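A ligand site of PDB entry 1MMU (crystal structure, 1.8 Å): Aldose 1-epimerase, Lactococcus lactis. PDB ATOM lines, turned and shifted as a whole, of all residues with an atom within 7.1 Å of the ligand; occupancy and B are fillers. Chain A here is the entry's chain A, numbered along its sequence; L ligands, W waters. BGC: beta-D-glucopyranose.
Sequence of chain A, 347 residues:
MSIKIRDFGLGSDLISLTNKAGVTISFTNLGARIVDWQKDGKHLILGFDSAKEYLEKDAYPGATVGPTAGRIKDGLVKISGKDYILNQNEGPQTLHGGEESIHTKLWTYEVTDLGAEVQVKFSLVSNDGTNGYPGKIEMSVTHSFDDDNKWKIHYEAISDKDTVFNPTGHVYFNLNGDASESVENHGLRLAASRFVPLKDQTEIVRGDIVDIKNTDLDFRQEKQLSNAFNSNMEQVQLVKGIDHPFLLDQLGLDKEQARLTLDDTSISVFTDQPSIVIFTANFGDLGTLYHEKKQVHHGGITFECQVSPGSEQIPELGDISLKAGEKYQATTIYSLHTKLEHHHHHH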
ATOM      1  N   ASP A  58       6.691  11.277  10.337  1.00  0.00           N
ATOM      2  CA  ASP A  58       7.561  12.374  10.726  1.00  0.00           C
ATOM      3  C   ASP A  58       8.941  11.762  10.651  1.00  0.00           C
ATOM      4  O   ASP A  58       9.223  10.784  11.324  1.00  0.00           O
ATOM      5  CB  ASP A  58       7.273  12.914  12.149  1.00  0.00           C
ATOM      6  CG  ASP A  58       8.166  14.087  12.525  1.00  0.00           C
ATOM      7  OD1 ASP A  58       9.052  14.511  11.795  1.00  0.00           O
ATOM      8  OD2 ASP A  58       7.891  14.610  13.722  1.00  0.00           O
ATOM      9  N   TYR A  60      11.750  13.199  11.490  1.00  0.00           N
ATOM     10  CA  TYR A  60      12.760  13.789  12.373  1.00  0.00           C
ATOM     11  C   TYR A  60      13.020  13.069  13.682  1.00  0.00           C
ATOM     12  O   TYR A  60      14.172  13.037  14.174  1.00  0.00           O
ATOM     13  CB  TYR A  60      12.467  15.286  12.649  1.00  0.00           C
ATOM     14  CG  TYR A  60      12.693  16.208  11.445  1.00  0.00           C
ATOM     15  CD1 TYR A  60      11.706  17.126  11.082  1.00  0.00           C
ATOM     16  CD2 TYR A  60      13.881  16.179  10.707  1.00  0.00           C
ATOM     17  CE1 TYR A  60      11.854  17.984   9.993  1.00  0.00           C
ATOM     18  CE2 TYR A  60      14.051  17.034   9.616  1.00  0.00           C
ATOM     19  CZ  TYR A  60      13.048  17.949   9.267  1.00  0.00           C
ATOM     20  OH  TYR A  60      13.192  18.813   8.191  1.00  0.00           O
ATOM     21  N   PRO A  61      11.973  12.503  14.287  1.00  0.00           N
ATOM     22  CA  PRO A  61      12.164  11.890  15.586  1.00  0.00           C
ATOM     23  C   PRO A  61      13.331  10.874  15.692  1.00  0.00           C
ATOM     24  O   PRO A  61      13.392   9.930  14.906  1.00  0.00           O
ATOM     25  CB  PRO A  61      10.808  11.267  15.926  1.00  0.00           C
ATOM     26  CG  PRO A  61       9.773  12.051  15.138  1.00  0.00           C
ATOM     27  CD  PRO A  61      10.511  12.470  13.888  1.00  0.00           C
ATOM     28  N   VAL A  65      20.176  14.917  12.359  1.00  0.00           N
ATOM     29  CA  VAL A  65      19.739  15.947  11.398  1.00  0.00           C
ATOM     30  C   VAL A  65      20.937  16.849  11.007  1.00  0.00           C
ATOM     31  O   VAL A  65      21.806  17.180  11.817  1.00  0.00           O
ATOM     32  CB  VAL A  65      18.524  16.819  11.839  1.00  0.00           C
ATOM     33  CG1 VAL A  65      17.223  15.998  11.938  1.00  0.00           C
ATOM     34  CG2 VAL A  65      18.837  17.537  13.160  1.00  0.00           C
ATOM     35  N   GLY A  70      18.552  23.031  12.663  1.00  0.00           N
ATOM     36  CA  GLY A  70      17.911  24.313  12.892  1.00  0.00           C
ATOM     37  C   GLY A  70      17.540  25.058  11.633  1.00  0.00           C
ATOM     38  O   GLY A  70      17.658  24.580  10.506  1.00  0.00           O
ATOM     39  N   ARG A  71      17.024  26.256  11.856  1.00  0.00           N
ATOM     40  CA  ARG A  71      16.595  27.083  10.745  1.00  0.00           C
ATOM     41  C   ARG A  71      17.649  28.107  10.318  1.00  0.00           C
ATOM     42  O   ARG A  71      18.177  28.873  11.170  1.00  0.00           O
ATOM     43  CB  ARG A  71      15.322  27.851  11.073  1.00  0.00           C
ATOM     44  CG  ARG A  71      14.099  26.991  11.171  1.00  0.00           C
ATOM     45  CD  ARG A  71      12.841  27.761  11.607  1.00  0.00           C
ATOM     46  NE  ARG A  71      11.744  26.783  11.644  1.00  0.00           N
ATOM     47  CZ  ARG A  71      11.482  26.016  12.688  1.00  0.00           C
ATOM     48  NH1 ARG A  71      12.152  26.130  13.843  1.00  0.00           N
ATOM     49  NH2 ARG A  71      10.510  25.127  12.557  1.00  0.00           N
ATOM     50  N   GLU A  90      11.270  25.134   4.198  1.00  0.00           N
ATOM     51  CA  GLU A  90      10.214  25.590   5.079  1.00  0.00           C
ATOM     52  C   GLU A  90      10.005  26.996   4.650  1.00  0.00           C
ATOM     53  O   GLU A  90      10.644  27.909   5.141  1.00  0.00           O
ATOM     54  CB  GLU A  90      10.674  25.501   6.533  1.00  0.00           C
ATOM     55  CG  GLU A  90       9.576  25.937   7.515  1.00  0.00           C
ATOM     56  CD  GLU A  90      10.049  26.057   8.948  1.00  0.00           C
ATOM     57  OE1 GLU A  90      10.762  26.945   9.339  1.00  0.00           O
ATOM     58  OE2 GLU A  90       9.602  25.123   9.735  1.00  0.00           O
ATOM     59  N   LEU A  95      15.467  24.260   6.857  1.00  0.00           N
ATOM     60  CA  LEU A  95      15.241  23.626   8.151  1.00  0.00           C
ATOM     61  C   LEU A  95      15.951  22.281   8.171  1.00  0.00           C
ATOM     62  O   LEU A  95      15.768  21.484   7.279  1.00  0.00           O
ATOM     63  CB  LEU A  95      13.729  23.421   8.437  1.00  0.00           C
ATOM     64  CG  LEU A  95      13.408  22.553   9.696  1.00  0.00           C
ATOM     65  CD1 LEU A  95      13.891  23.246  10.981  1.00  0.00           C
ATOM     66  CD2 LEU A  95      11.901  22.316   9.828  1.00  0.00           C
ATOM     67  N   HIS A  96      16.808  22.101   9.169  1.00  0.00           N
ATOM     68  CA  HIS A  96      17.536  20.858   9.319  1.00  0.00           C
ATOM     69  C   HIS A  96      18.111  20.306   8.028  1.00  0.00           C
ATOM     70  O   HIS A  96      17.811  19.148   7.621  1.00  0.00           O
ATOM     71  CB  HIS A  96      16.550  19.795   9.866  1.00  0.00           C
ATOM     72  CG  HIS A  96      16.126  20.117  11.253  1.00  0.00           C
ATOM     73  ND1 HIS A  96      16.952  20.878  12.063  1.00  0.00           N
ATOM     74  CD2 HIS A  96      15.012  19.773  11.943  1.00  0.00           C
ATOM     75  CE1 HIS A  96      16.321  20.980  13.225  1.00  0.00           C
ATOM     76  NE2 HIS A  96      15.150  20.331  13.195  1.00  0.00           N
ATOM     77  N   HIS A 170      17.992  14.375  17.191  1.00  0.00           N
ATOM     78  CA  HIS A 170      16.656  14.818  17.369  1.00  0.00           C
ATOM     79  C   HIS A 170      15.758  13.899  18.179  1.00  0.00           C
ATOM     80  O   HIS A 170      14.520  13.880  18.008  1.00  0.00           O
ATOM     81  CB  HIS A 170      16.048  15.210  16.000  1.00  0.00           C
ATOM     82  CG  HIS A 170      14.908  16.185  16.064  1.00  0.00           C
ATOM     83  ND1 HIS A 170      13.708  15.893  16.721  1.00  0.00           N
ATOM     84  CD2 HIS A 170      14.797  17.426  15.502  1.00  0.00           C
ATOM     85  CE1 HIS A 170      12.921  16.956  16.557  1.00  0.00           C
ATOM     86  NE2 HIS A 170      13.554  17.893  15.829  1.00  0.00           N
ATOM     87  N   TYR A 172      13.299  12.558  20.968  1.00  0.00           N
ATOM     88  CA  TYR A 172      12.218  13.135  21.785  1.00  0.00           C
ATOM     89  C   TYR A 172      12.058  12.252  23.041  1.00  0.00           C
ATOM     90  O   TYR A 172      11.864  11.042  22.936  1.00  0.00           O
ATOM     91  CB  TYR A 172      10.826  13.125  21.118  1.00  0.00           C
ATOM     92  CG  TYR A 172      10.592  14.135  20.035  1.00  0.00           C
ATOM     93  CD1 TYR A 172      10.831  13.803  18.700  1.00  0.00           C
ATOM     94  CD2 TYR A 172      10.039  15.376  20.357  1.00  0.00           C
ATOM     95  CE1 TYR A 172      10.541  14.739  17.694  1.00  0.00           C
ATOM     96  CE2 TYR A 172       9.766  16.333  19.377  1.00  0.00           C
ATOM     97  CZ  TYR A 172      10.013  15.990  18.041  1.00  0.00           C
ATOM     98  OH  TYR A 172       9.740  16.886  17.053  1.00  0.00           O
ATOM     99  N   LEU A 198      12.682  33.988  19.144  1.00  0.00           N
ATOM    100  CA  LEU A 198      12.395  33.853  17.730  1.00  0.00           C
ATOM    101  C   LEU A 198      11.705  35.122  17.253  1.00  0.00           C
ATOM    102  O   LEU A 198      11.063  35.796  18.031  1.00  0.00           O
ATOM    103  CB  LEU A 198      11.509  32.641  17.493  1.00  0.00           C
ATOM    104  CG  LEU A 198      12.136  31.405  18.134  1.00  0.00           C
ATOM    105  CD1 LEU A 198      11.187  30.227  17.969  1.00  0.00           C
ATOM    106  CD2 LEU A 198      13.535  31.127  17.559  1.00  0.00           C
ATOM    107  N   GLU A 203       9.740  31.608  12.811  1.00  0.00           N
ATOM    108  CA  GLU A 203      10.745  30.984  13.635  1.00  0.00           C
ATOM    109  C   GLU A 203      12.181  31.318  13.400  1.00  0.00           C
ATOM    110  O   GLU A 203      13.059  30.662  13.955  1.00  0.00           O
ATOM    111  CB  GLU A 203      10.453  29.462  13.810  1.00  0.00           C
ATOM    112  CG  GLU A 203       9.093  29.238  14.531  1.00  0.00           C
ATOM    113  CD  GLU A 203       8.446  27.876  14.408  1.00  0.00           C
ATOM    114  OE1 GLU A 203       7.939  27.481  13.374  1.00  0.00           O
ATOM    115  OE2 GLU A 203       8.415  27.181  15.518  1.00  0.00           O
ATOM    116  N   VAL A 239       5.096  30.097  20.251  1.00  0.00           N
ATOM    117  CA  VAL A 239       5.233  28.687  19.741  1.00  0.00           C
ATOM    118  C   VAL A 239       4.301  27.682  20.351  1.00  0.00           C
ATOM    119  O   VAL A 239       4.220  26.525  19.880  1.00  0.00           O
ATOM    120  CB  VAL A 239       6.681  28.161  19.858  1.00  0.00           C
ATOM    121  CG1 VAL A 239       7.668  29.109  19.152  1.00  0.00           C
ATOM    122  CG2 VAL A 239       7.088  28.051  21.328  1.00  0.00           C
ATOM    123  N   ILE A 242       7.679  25.417  23.994  1.00  0.00           N
ATOM    124  CA  ILE A 242       9.106  25.761  23.849  1.00  0.00           C
ATOM    125  C   ILE A 242       9.582  25.234  22.489  1.00  0.00           C
ATOM    126  O   ILE A 242       9.148  24.171  22.029  1.00  0.00           O
ATOM    127  CB  ILE A 242       9.944  25.176  24.975  1.00  0.00           C
ATOM    128  CG1 ILE A 242       9.199  25.370  26.331  1.00  0.00           C
ATOM    129  CG2 ILE A 242      11.369  25.772  24.964  1.00  0.00           C
ATOM    130  CD1 ILE A 242       9.989  24.838  27.531  1.00  0.00           C
ATOM    131  N   ASP A 243      10.415  26.038  21.841  1.00  0.00           N
ATOM    132  CA  ASP A 243      10.988  25.763  20.522  1.00  0.00           C
ATOM    133  C   ASP A 243      12.134  26.724  20.399  1.00  0.00           C
ATOM    134  O   ASP A 243      12.223  27.584  19.501  1.00  0.00           O
ATOM    135  CB  ASP A 243       9.927  26.014  19.411  1.00  0.00           C
ATOM    136  CG  ASP A 243      10.315  25.242  18.164  1.00  0.00           C
ATOM    137  OD1 ASP A 243      11.364  24.628  18.069  1.00  0.00           O
ATOM    138  OD2 ASP A 243       9.387  25.206  17.227  1.00  0.00           O
ATOM    139  N   VAL A 277      18.899  23.110  22.008  1.00  0.00           N
ATOM    140  CA  VAL A 277      17.657  23.557  21.423  1.00  0.00           C
ATOM    141  C   VAL A 277      16.548  22.641  21.950  1.00  0.00           C
ATOM    142  O   VAL A 277      16.611  21.389  21.830  1.00  0.00           O
ATOM    143  CB  VAL A 277      17.709  23.612  19.887  1.00  0.00           C
ATOM    144  CG1 VAL A 277      16.288  23.851  19.308  1.00  0.00           C
ATOM    145  CG2 VAL A 277      18.692  24.698  19.426  1.00  0.00           C
ATOM    146  N   PHE A 279      12.585  21.582  22.062  1.00  0.00           N
ATOM    147  CA  PHE A 279      11.303  21.581  21.367  1.00  0.00           C
ATOM    148  C   PHE A 279      10.319  20.652  22.080  1.00  0.00           C
ATOM    149  O   PHE A 279      10.543  19.438  22.258  1.00  0.00           O
ATOM    150  CB  PHE A 279      11.473  21.286  19.854  1.00  0.00           C
ATOM    151  CG  PHE A 279      10.128  21.205  19.164  1.00  0.00           C
ATOM    152  CD1 PHE A 279       9.267  22.319  19.177  1.00  0.00           C
ATOM    153  CD2 PHE A 279       9.692  20.018  18.574  1.00  0.00           C
ATOM    154  CE1 PHE A 279       8.017  22.263  18.569  1.00  0.00           C
ATOM    155  CE2 PHE A 279       8.448  19.949  17.943  1.00  0.00           C
ATOM    156  CZ  PHE A 279       7.619  21.069  17.960  1.00  0.00           C
ATOM    157  N   ASN A 282       4.991  20.865  20.107  1.00  0.00           N
ATOM    158  CA  ASN A 282       3.857  21.792  20.124  1.00  0.00           C
ATOM    159  C   ASN A 282       2.880  21.537  18.974  1.00  0.00           C
ATOM    160  O   ASN A 282       2.359  22.448  18.347  1.00  0.00           O
ATOM    161  CB  ASN A 282       4.397  23.250  20.151  1.00  0.00           C
ATOM    162  CG  ASN A 282       5.480  23.415  21.195  1.00  0.00           C
ATOM    163  OD1 ASN A 282       5.345  22.906  22.317  1.00  0.00           O
ATOM    164  ND2 ASN A 282       6.556  24.107  20.857  1.00  0.00           N
ATOM    165  N   PHE A 283       2.608  20.270  18.749  1.00  0.00           N
ATOM    166  CA  PHE A 283       1.741  19.851  17.642  1.00  0.00           C
ATOM    167  C   PHE A 283       0.234  20.067  17.697  1.00  0.00           C
ATOM    168  O   PHE A 283      -0.465  19.760  16.709  1.00  0.00           O
ATOM    169  CB  PHE A 283       2.015  18.392  17.233  1.00  0.00           C
ATOM    170  CG  PHE A 283       3.460  18.217  16.834  1.00  0.00           C
ATOM    171  CD1 PHE A 283       4.301  17.423  17.613  1.00  0.00           C
ATOM    172  CD2 PHE A 283       3.988  18.843  15.692  1.00  0.00           C
ATOM    173  CE1 PHE A 283       5.635  17.239  17.243  1.00  0.00           C
ATOM    174  CE2 PHE A 283       5.324  18.677  15.328  1.00  0.00           C
ATOM    175  CZ  PHE A 283       6.150  17.864  16.107  1.00  0.00           C
ATOM    176  N   LEU A 286      -2.650  17.649  15.945  1.00  0.00           N
ATOM    177  CA  LEU A 286      -2.145  16.805  14.931  1.00  0.00           C
ATOM    178  C   LEU A 286      -2.371  15.295  15.263  1.00  0.00           C
ATOM    179  O   LEU A 286      -2.807  14.508  14.446  1.00  0.00           O
ATOM    180  CB  LEU A 286      -0.710  17.250  14.560  1.00  0.00           C
ATOM    181  CG  LEU A 286      -0.052  16.394  13.507  1.00  0.00           C
ATOM    182  CD1 LEU A 286      -0.784  16.610  12.189  1.00  0.00           C
ATOM    183  CD2 LEU A 286       1.387  16.843  13.365  1.00  0.00           C
ATOM    184  N   THR A 302      12.577  17.630  23.132  1.00  0.00           N
ATOM    185  CA  THR A 302      13.924  17.341  22.632  1.00  0.00           C
ATOM    186  C   THR A 302      15.002  18.058  23.436  1.00  0.00           C
ATOM    187  O   THR A 302      14.707  18.972  24.190  1.00  0.00           O
ATOM    188  CB  THR A 302      14.081  17.794  21.175  1.00  0.00           C
ATOM    189  OG1 THR A 302      14.053  19.210  21.213  1.00  0.00           O
ATOM    190  CG2 THR A 302      12.953  17.302  20.259  1.00  0.00           C
ATOM    191  N   GLU A 304      18.306  19.141  21.719  1.00  0.00           N
ATOM    192  CA  GLU A 304      19.188  19.202  20.535  1.00  0.00           C
ATOM    193  C   GLU A 304      20.440  19.989  20.847  1.00  0.00           C
ATOM    194  O   GLU A 304      20.436  21.214  20.848  1.00  0.00           O
ATOM    195  CB  GLU A 304      18.456  19.723  19.289  1.00  0.00           C
ATOM    196  CG  GLU A 304      17.227  18.874  18.934  1.00  0.00           C
ATOM    197  CD  GLU A 304      16.311  19.657  18.027  1.00  0.00           C
ATOM    198  OE1 GLU A 304      16.621  20.065  16.928  1.00  0.00           O
ATOM    199  OE2 GLU A 304      15.150  19.914  18.563  1.00  0.00           O
HETATM  200  C2  BGC L   1       8.340  22.289  13.980  1.00  0.00           C
HETATM  201  C3  BGC L   1       8.148  20.784  13.864  1.00  0.00           C
HETATM  202  C4  BGC L   1       9.476  20.125  13.514  1.00  0.00           C
HETATM  203  C5  BGC L   1      10.543  20.591  14.520  1.00  0.00           C
HETATM  204  C6  BGC L   1      11.921  20.029  14.154  1.00  0.00           C
HETATM  205  C1  BGC L   1       9.439  22.656  14.957  1.00  0.00           C
HETATM  206  O1  BGC L   1       9.521  24.081  14.967  1.00  0.00           O
HETATM  207  O2  BGC L   1       7.088  22.872  14.373  1.00  0.00           O
HETATM  208  O3  BGC L   1       7.169  20.441  12.844  1.00  0.00           O
HETATM  209  O4  BGC L   1       9.375  18.703  13.588  1.00  0.00           O
HETATM  210  O5  BGC L   1      10.664  22.027  14.550  1.00  0.00           O
HETATM  211  O6  BGC L   1      12.869  20.488  15.093  1.00  0.00           O
HETATM  212  O   HOH W   1       6.528  25.381  13.450  1.00  0.00           O
HETATM  213  O   HOH W   2      12.417  23.587  15.703  1.00  0.00           O
HETATM  214  O   HOH W   3       5.255  23.091  16.634  1.00  0.00           O
HETATM  215  O   HOH W   4       4.128  19.297  11.631  1.00  0.00           O
HETATM  216  O   HOH W   5       7.630  17.122  12.160  1.00  0.00           O
HETATM  217  O   HOH W   6       4.605  21.440  13.122  1.00  0.00           O
HETATM  218  O   HOH W   7       7.978  20.714  10.504  1.00  0.00           O
HETATM  219  O   HOH W   8       9.653  16.228  14.648  1.00  0.00           O
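N of Tyr 60 sits at hydrogen-bond distance from OD1 of Asp 58, 3.0 Å away. ND1 of His 96 is in hydrogen-bond range of N of Gly 70 (2.7 Å). The guanidinium group (NH2) of Arg 71 is in salt-bridge range of the side-chain carboxylate (OE1) of Glu 203. NE of Arg 71 is in salt-bridge range of OE1 of Glu 90. The backbone carbonyl oxygen of Phe 279 lies within hydrogen-bond range of the backbone NH of Thr 302, at 2.9 Å.
CD1 of Tyr 60 touches O4 of the ligand, at 3.8 Å. Tyr 172 touches the ligand. CZ of Phe 279 touches C1 of the ligand (3.9 Å). CE2 of Phe 283 touches O3 of the ligand, 3.6 Å away. Hydrophobic or aromatic side chains that line the ligand: Tyr 60, His 96, His 170, Phe 279 and Phe 283. Nine residues have an atom within 4 Å of the ligand: Tyr 60, Arg 71, His 96, His 170, Tyr 172, Glu 203, Asp 243, Phe 279 and Phe 283.
OD2 of Asp 243 sits at hydrogen-bond distance from O1 of the ligand (2.5 Å). An oxygen (O6) of the ligand sits at hydrogen-bond distance from a ring nitrogen (NE2) of His 170 (2.8 Å). The side-chain carboxylate (OE2) of Glu 203 sits at hydrogen-bond distance from an oxygen (O1) of the ligand, 3.3 Å away. An oxygen (O1) of the ligand is in hydrogen-bond range of the guanidinium group (NH2) of Arg 71 (2.8 Å). An oxygen (O6) of the ligand is in hydrogen-bond range of a ring nitrogen (NE2) of His 96 (3.0 Å).
Water W2 lies within hydrogen-bond range of O5 of the ligand (2.6 Å), OD1 of Asp 243 (2.8 Å) and NH1 of Arg 71 (3.2 Å). Water W8 lies within hydrogen-bond range of the side-chain hydroxyl (OH) of Tyr 172 (2.5 Å), the side-chain carboxylate (OD2) of Asp 58 (2.6 Å) and an oxygen (O4) of the ligand (2.7 Å). Water W1 lies within hydrogen-bond range of OE1 of Glu 203 (2.5 Å) and O2 of the ligand (2.7 Å). Water W5 bridges O4 of the ligand (2.8 Å) and OD2 of Asp 58 (3.0 Å). Water W3 lies within hydrogen-bond range of O2 of the ligand and O of Asn 282.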
